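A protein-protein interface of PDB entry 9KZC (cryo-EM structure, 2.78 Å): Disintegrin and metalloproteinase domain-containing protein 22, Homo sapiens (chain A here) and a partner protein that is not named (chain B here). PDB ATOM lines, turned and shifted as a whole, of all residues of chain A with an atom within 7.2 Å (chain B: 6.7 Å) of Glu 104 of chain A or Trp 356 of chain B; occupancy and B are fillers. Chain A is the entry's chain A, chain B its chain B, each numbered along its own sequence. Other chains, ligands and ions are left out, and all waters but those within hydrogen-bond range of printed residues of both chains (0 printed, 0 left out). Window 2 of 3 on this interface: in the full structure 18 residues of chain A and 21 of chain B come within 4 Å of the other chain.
The backbone NH of Glu 104 of chain A sits at hydrogen-bond distance from the backbone carbonyl oxygen of Glu 71 of chain A (3.0 Å). N of Phe 103 of chain A sits at hydrogen-bond distance from OE1 of Glu 127 of chain A (2.7 Å). OG of Ser 105 of chain A is in hydrogen-bond range of O of Arg 107 of chain A (3.2 Å).
Of the 10 printed residues of chain B, 4 touch a printed residue of chain A. Hydrophobic or aromatic side chains of chain B within 4 Å of the printed part of chain A: Ala 334, Trp 356 and Tyr 357. Among the printed residues, Asp or Glu carboxylates within 4 Å of a Lys or Arg side-chain nitrogen of the other chain: Glu 127 of chain A with Lys 333 of chain B (3.1 Å).
Glu 104 of chain A touches just one residue of chain B: Trp 356. Trp 356 of chain B touches just these residues of chain A: Gln 102 (3.2 Å), Glu 104 (3.3 Å), Ser 105 (3.3 Å) and Ser 106 (3.6 Å). Of the printed residues of chain B, Arg 107 of chain A touches Lys 333 (3.7 Å). Of the printed residues of chain B, Glu 127 of chain A touches Lys 333. Of the printed residues of chain A, Tyr 357 of chain B touches Gln 102. Ser 332 of chain B touches none of the printed residues of chain A. The nearest residue of chain B that does not touch Glu 104 of chain A is Lys 333 of chain B (4.3 Å). The nearest residue of chain A that does not touch Trp 356 of chain B is Phe 103 of chain A (4.03 Å). The nearest printed residue of chain B that does not touch Ser 105 of chain A is Ala 334 of chain B (5.3 Å).
Among the printed residues, pairs that only touch across the chains: Ser 106 of chain A with Ala 334 of chain B (3.1 Å), Gln 102 of chain A with Tyr 357 of chain B (3.2 Å), Ser 105 of chain A with Trp 356 of chain B (3.3 Å), Ser 106 of chain A with Trp 356 of chain B (3.6 Å), Arg 107 of chain A with Lys 333 of chain B (3.7 Å) and Ser 106 of chain A with Lys 333 of chain B (3.7 Å).
NE2 of Gln 102 of chain A is in hydrogen-bond range of O of Trp 356 of chain B, at 3.2 Å. The side-chain amino group (NZ) of Lys 333 of chain B is in hydrogen-bond range of the backbone carbonyl oxygen (O) of Phe 103 of chain A (2.4 Å). The backbone carbonyl oxygen (O) of Glu 104 of chain A sits close to the indole nitrogen (NE1) of Trp 356 of chain B (3.5 Å). The side-chain amino group (NZ) of Lys 333 of chain B lies close to the backbone carbonyl oxygen (O) of Ser 105 of chain A (3.4 Å). OE1 of Glu 127 of chain A lies within salt-bridge range of NZ of Lys 333 of chain B, at 3.1 Å.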
ATOM      1  N   SER A  70      10.351  20.494  15.152  1.00  0.00           N
ATOM      2  CA  SER A  70      11.522  19.634  15.133  1.00  0.00           C
ATOM      3  C   SER A  70      11.171  18.263  14.567  1.00  0.00           C
ATOM      4  O   SER A  70      10.016  17.831  14.585  1.00  0.00           O
ATOM      5  CB  SER A  70      12.106  19.485  16.540  1.00  0.00           C
ATOM      6  OG  SER A  70      13.038  18.421  16.596  1.00  0.00           O
ATOM      7  N   GLU A  71      12.196  17.579  14.056  1.00  0.00           N
ATOM      8  CA  GLU A  71      12.018  16.216  13.573  1.00  0.00           C
ATOM      9  C   GLU A  71      11.831  15.217  14.705  1.00  0.00           C
ATOM     10  O   GLU A  71      11.424  14.080  14.445  1.00  0.00           O
ATOM     11  CB  GLU A  71      13.209  15.805  12.704  1.00  0.00           C
ATOM     12  CG  GLU A  71      14.408  15.296  13.487  1.00  0.00           C
ATOM     13  CD  GLU A  71      15.246  16.419  14.066  1.00  0.00           C
ATOM     14  OE1 GLU A  71      15.090  17.573  13.616  1.00  0.00           O
ATOM     15  OE2 GLU A  71      16.063  16.145  14.970  1.00  0.00           O
ATOM     16  N   ASN A  72      12.120  15.610  15.944  1.00  0.00           N
ATOM     17  CA  ASN A  72      11.862  14.767  17.101  1.00  0.00           C
ATOM     18  C   ASN A  72      10.434  14.994  17.573  1.00  0.00           C
ATOM     19  O   ASN A  72      10.091  16.126  17.941  1.00  0.00           O
ATOM     20  CB  ASN A  72      12.841  15.083  18.220  1.00  0.00           C
ATOM     21  CG  ASN A  72      12.932  13.975  19.253  1.00  0.00           C
ATOM     22  OD1 ASN A  72      12.017  13.169  19.403  1.00  0.00           O
ATOM     23  ND2 ASN A  72      14.043  13.937  19.977  1.00  0.00           N
ATOM     24  N   PRO A  73       9.573  13.974  17.568  1.00  0.00           N
ATOM     25  CA  PRO A  73       8.182  14.193  17.997  1.00  0.00           C
ATOM     26  C   PRO A  73       8.047  14.640  19.442  1.00  0.00           C
ATOM     27  O   PRO A  73       7.092  15.353  19.766  1.00  0.00           O
ATOM     28  CB  PRO A  73       7.526  12.825  17.764  1.00  0.00           C
ATOM     29  CG  PRO A  73       8.652  11.857  17.758  1.00  0.00           C
ATOM     30  CD  PRO A  73       9.809  12.583  17.152  1.00  0.00           C
ATOM     31  N   GLN A 102       7.468  15.354   8.459  1.00  0.00           N
ATOM     32  CA  GLN A 102       7.599  13.940   8.774  1.00  0.00           C
ATOM     33  C   GLN A 102       8.587  13.776   9.917  1.00  0.00           C
ATOM     34  O   GLN A 102       9.706  14.297   9.855  1.00  0.00           O
ATOM     35  CB  GLN A 102       8.060  13.139   7.554  1.00  0.00           C
ATOM     36  CG  GLN A 102       8.294  11.667   7.841  1.00  0.00           C
ATOM     37  CD  GLN A 102       9.343  11.056   6.936  1.00  0.00           C
ATOM     38  OE1 GLN A 102      10.543  11.168   7.192  1.00  0.00           O
ATOM     39  NE2 GLN A 102       8.896  10.400   5.874  1.00  0.00           N
ATOM     40  N   PHE A 103       8.172  13.059  10.954  1.00  0.00           N
ATOM     41  CA  PHE A 103       9.033  12.817  12.099  1.00  0.00           C
ATOM     42  C   PHE A 103      10.096  11.780  11.759  1.00  0.00           C
ATOM     43  O   PHE A 103       9.878  10.873  10.951  1.00  0.00           O
ATOM     44  CB  PHE A 103       8.209  12.355  13.300  1.00  0.00           C
ATOM     45  CG  PHE A 103       7.278  13.407  13.833  1.00  0.00           C
ATOM     46  CD1 PHE A 103       7.726  14.698  14.055  1.00  0.00           C
ATOM     47  CD2 PHE A 103       5.956  13.104  14.110  1.00  0.00           C
ATOM     48  CE1 PHE A 103       6.873  15.667  14.545  1.00  0.00           C
ATOM     49  CE2 PHE A 103       5.099  14.069  14.599  1.00  0.00           C
ATOM     50  CZ  PHE A 103       5.558  15.353  14.816  1.00  0.00           C
ATOM     51  N   GLU A 104      11.258  11.924  12.391  1.00  0.00           N
ATOM     52  CA  GLU A 104      12.407  11.052  12.158  1.00  0.00           C
ATOM     53  C   GLU A 104      12.520   9.972  13.223  1.00  0.00           C
ATOM     54  O   GLU A 104      13.622   9.629  13.660  1.00  0.00           O
ATOM     55  CB  GLU A 104      13.689  11.873  12.088  1.00  0.00           C
ATOM     56  CG  GLU A 104      13.814  12.708  10.828  1.00  0.00           C
ATOM     57  CD  GLU A 104      15.245  12.827  10.350  1.00  0.00           C
ATOM     58  OE1 GLU A 104      16.147  12.312  11.042  1.00  0.00           O
ATOM     59  OE2 GLU A 104      15.467  13.435   9.283  1.00  0.00           O
ATOM     60  N   SER A 105      11.391   9.431  13.668  1.00  0.00           N
ATOM     61  CA  SER A 105      11.361   8.400  14.691  1.00  0.00           C
ATOM     62  C   SER A 105      10.475   7.250  14.225  1.00  0.00           C
ATOM     63  O   SER A 105       9.840   7.310  13.169  1.00  0.00           O
ATOM     64  CB  SER A 105      10.860   8.963  16.026  1.00  0.00           C
ATOM     65  OG  SER A 105       9.528   9.423  15.904  1.00  0.00           O
ATOM     66  N   SER A 106      10.443   6.189  15.034  1.00  0.00           N
ATOM     67  CA  SER A 106       9.592   5.040  14.751  1.00  0.00           C
ATOM     68  C   SER A 106       8.109   5.373  14.838  1.00  0.00           C
ATOM     69  O   SER A 106       7.290   4.652  14.262  1.00  0.00           O
ATOM     70  CB  SER A 106       9.920   3.902  15.718  1.00  0.00           C
ATOM     71  OG  SER A 106       8.945   2.879  15.651  1.00  0.00           O
ATOM     72  N   ARG A 107       7.749   6.443  15.537  1.00  0.00           N
ATOM     73  CA  ARG A 107       6.358   6.787  15.787  1.00  0.00           C
ATOM     74  C   ARG A 107       5.911   7.907  14.857  1.00  0.00           C
ATOM     75  O   ARG A 107       6.679   8.824  14.555  1.00  0.00           O
ATOM     76  CB  ARG A 107       6.161   7.207  17.245  1.00  0.00           C
ATOM     77  CG  ARG A 107       7.156   8.250  17.727  1.00  0.00           C
ATOM     78  CD  ARG A 107       6.819   8.743  19.124  1.00  0.00           C
ATOM     79  NE  ARG A 107       7.464   7.949  20.162  1.00  0.00           N
ATOM     80  CZ  ARG A 107       7.035   7.863  21.414  1.00  0.00           C
ATOM     81  NH1 ARG A 107       5.952   8.504  21.819  1.00  0.00           N
ATOM     82  NH2 ARG A 107       7.710   7.113  22.281  1.00  0.00           N
ATOM     83  N   GLU A 127       1.816  13.570  12.485  1.00  0.00           N
ATOM     84  CA  GLU A 127       2.445  13.912  11.219  1.00  0.00           C
ATOM     85  C   GLU A 127       1.493  13.648  10.057  1.00  0.00           C
ATOM     86  O   GLU A 127       0.569  12.836  10.146  1.00  0.00           O
ATOM     87  CB  GLU A 127       3.746  13.129  11.028  1.00  0.00           C
ATOM     88  CG  GLU A 127       3.566  11.736  10.458  1.00  0.00           C
ATOM     89  CD  GLU A 127       4.887  11.041  10.200  1.00  0.00           C
ATOM     90  OE1 GLU A 127       5.928  11.560  10.650  1.00  0.00           O
ATOM     91  OE2 GLU A 127       4.884   9.978   9.549  1.00  0.00           O
ATOM     92  N   SER B 332       6.565   0.278   7.138  1.00  0.00           N
ATOM     93  CA  SER B 332       6.509   0.871   8.463  1.00  0.00           C
ATOM     94  C   SER B 332       7.613   1.910   8.616  1.00  0.00           C
ATOM     95  O   SER B 332       8.652   1.837   7.956  1.00  0.00           O
ATOM     96  CB  SER B 332       6.645  -0.198   9.550  1.00  0.00           C
ATOM     97  OG  SER B 332       7.796  -0.994   9.335  1.00  0.00           O
ATOM     98  N   LYS B 333       7.367   2.893   9.484  1.00  0.00           N
ATOM     99  CA  LYS B 333       8.392   3.891   9.773  1.00  0.00           C
ATOM    100  C   LYS B 333       9.584   3.268  10.488  1.00  0.00           C
ATOM    101  O   LYS B 333      10.737   3.602  10.191  1.00  0.00           O
ATOM    102  CB  LYS B 333       7.802   5.024  10.609  1.00  0.00           C
ATOM    103  CG  LYS B 333       6.846   5.925   9.856  1.00  0.00           C
ATOM    104  CD  LYS B 333       6.740   7.281  10.527  1.00  0.00           C
ATOM    105  CE  LYS B 333       8.050   8.039  10.430  1.00  0.00           C
ATOM    106  NZ  LYS B 333       8.006   9.322  11.175  1.00  0.00           N
ATOM    107  N   ALA B 334       9.325   2.367  11.437  1.00  0.00           N
ATOM    108  CA  ALA B 334      10.405   1.750  12.199  1.00  0.00           C
ATOM    109  C   ALA B 334      11.293   0.882  11.317  1.00  0.00           C
ATOM    110  O   ALA B 334      12.521   0.895  11.459  1.00  0.00           O
ATOM    111  CB  ALA B 334       9.829   0.926  13.347  1.00  0.00           C
ATOM    112  N   GLY B 335      10.695   0.117  10.407  1.00  0.00           N
ATOM    113  CA  GLY B 335      11.454  -0.767   9.541  1.00  0.00           C
ATOM    114  C   GLY B 335      11.911  -0.054   8.279  1.00  0.00           C
ATOM    115  O   GLY B 335      11.151   0.680   7.653  1.00  0.00           O
ATOM    116  N   PHE B 336      13.164  -0.290   7.912  1.00  0.00           N
ATOM    117  CA  PHE B 336      13.768   0.356   6.758  1.00  0.00           C
ATOM    118  C   PHE B 336      13.868  -0.618   5.592  1.00  0.00           C
ATOM    119  O   PHE B 336      13.982  -1.832   5.780  1.00  0.00           O
ATOM    120  CB  PHE B 336      15.161   0.897   7.094  1.00  0.00           C
ATOM    121  CG  PHE B 336      15.187   1.835   8.269  1.00  0.00           C
ATOM    122  CD1 PHE B 336      14.070   2.580   8.612  1.00  0.00           C
ATOM    123  CD2 PHE B 336      16.334   1.970   9.032  1.00  0.00           C
ATOM    124  CE1 PHE B 336      14.097   3.438   9.690  1.00  0.00           C
ATOM    125  CE2 PHE B 336      16.365   2.830  10.113  1.00  0.00           C
ATOM    126  CZ  PHE B 336      15.246   3.564  10.442  1.00  0.00           C
ATOM    127  N   HIS B 354      15.878   3.822   2.784  1.00  0.00           N
ATOM    128  CA  HIS B 354      14.914   4.918   2.855  1.00  0.00           C
ATOM    129  C   HIS B 354      14.356   4.930   4.278  1.00  0.00           C
ATOM    130  O   HIS B 354      13.323   4.314   4.555  1.00  0.00           O
ATOM    131  CB  HIS B 354      13.829   4.713   1.800  1.00  0.00           C
ATOM    132  CG  HIS B 354      13.073   5.951   1.441  1.00  0.00           C
ATOM    133  ND1 HIS B 354      11.865   5.917   0.780  1.00  0.00           N
ATOM    134  CD2 HIS B 354      13.394   7.260   1.568  1.00  0.00           C
ATOM    135  CE1 HIS B 354      11.449   7.151   0.561  1.00  0.00           C
ATOM    136  NE2 HIS B 354      12.360   7.985   1.028  1.00  0.00           N
ATOM    137  N   ALA B 355      15.043   5.630   5.178  1.00  0.00           N
ATOM    138  CA  ALA B 355      14.732   5.565   6.599  1.00  0.00           C
ATOM    139  C   ALA B 355      13.527   6.429   6.951  1.00  0.00           C
ATOM    140  O   ALA B 355      13.368   7.537   6.436  1.00  0.00           O
ATOM    141  CB  ALA B 355      15.939   6.004   7.428  1.00  0.00           C
ATOM    142  N   TRP B 356      12.688   5.913   7.854  1.00  0.00           N
ATOM    143  CA  TRP B 356      11.500   6.586   8.377  1.00  0.00           C
ATOM    144  C   TRP B 356      10.430   6.813   7.319  1.00  0.00           C
ATOM    145  O   TRP B 356       9.569   7.681   7.488  1.00  0.00           O
ATOM    146  CB  TRP B 356      11.852   7.919   9.050  1.00  0.00           C
ATOM    147  CG  TRP B 356      13.059   7.857   9.930  1.00  0.00           C
ATOM    148  CD1 TRP B 356      14.179   8.627   9.835  1.00  0.00           C
ATOM    149  CD2 TRP B 356      13.265   6.986  11.048  1.00  0.00           C
ATOM    150  NE1 TRP B 356      15.073   8.286  10.819  1.00  0.00           N
ATOM    151  CE2 TRP B 356      14.535   7.280  11.577  1.00  0.00           C
ATOM    152  CE3 TRP B 356      12.500   5.983  11.651  1.00  0.00           C
ATOM    153  CZ2 TRP B 356      15.057   6.610  12.679  1.00  0.00           C
ATOM    154  CZ3 TRP B 356      13.021   5.319  12.742  1.00  0.00           C
ATOM    155  CH2 TRP B 356      14.286   5.635  13.247  1.00  0.00           C
ATOM    156  N   TYR B 357      10.453   6.050   6.232  1.00  0.00           N
ATOM    157  CA  TYR B 357       9.455   6.147   5.181  1.00  0.00           C
ATOM    158  C   TYR B 357       8.671   4.846   5.083  1.00  0.00           C
ATOM    159  O   TYR B 357       9.183   3.767   5.395  1.00  0.00           O
ATOM    160  CB  TYR B 357      10.101   6.469   3.832  1.00  0.00           C
ATOM    161  CG  TYR B 357      10.495   7.918   3.666  1.00  0.00           C
ATOM    162  CD1 TYR B 357      11.717   8.380   4.126  1.00  0.00           C
ATOM    163  CD2 TYR B 357       9.650   8.819   3.039  1.00  0.00           C
ATOM    164  CE1 TYR B 357      12.087   9.698   3.974  1.00  0.00           C
ATOM    165  CE2 TYR B 357      10.011  10.141   2.880  1.00  0.00           C
ATOM    166  CZ  TYR B 357      11.230  10.575   3.350  1.00  0.00           C
ATOM    167  OH  TYR B 357      11.594  11.892   3.195  1.00  0.00           O
ATOM    168  N   ARG B 358       7.418   4.960   4.647  1.00  0.00           N
ATOM    169  CA  ARG B 358       6.532   3.808   4.498  1.00  0.00           C
ATOM    170  C   ARG B 358       6.573   3.354   3.043  1.00  0.00           C
ATOM    171  O   ARG B 358       5.700   3.666   2.235  1.00  0.00           O
ATOM    172  CB  ARG B 358       5.120   4.164   4.945  1.00  0.00           C
ATOM    173  CG  ARG B 358       5.047   4.782   6.329  1.00  0.00           C
ATOM    174  CD  ARG B 358       3.634   5.230   6.651  1.00  0.00           C
ATOM    175  NE  ARG B 358       3.508   5.699   8.025  1.00  0.00           N
ATOM    176  CZ  ARG B 358       3.213   4.922   9.057  1.00  0.00           C
ATOM    177  NH1 ARG B 358       3.017   3.622   8.909  1.00  0.00           N
ATOM    178  NH2 ARG B 358       3.110   5.461  10.267  1.00  0.00           N
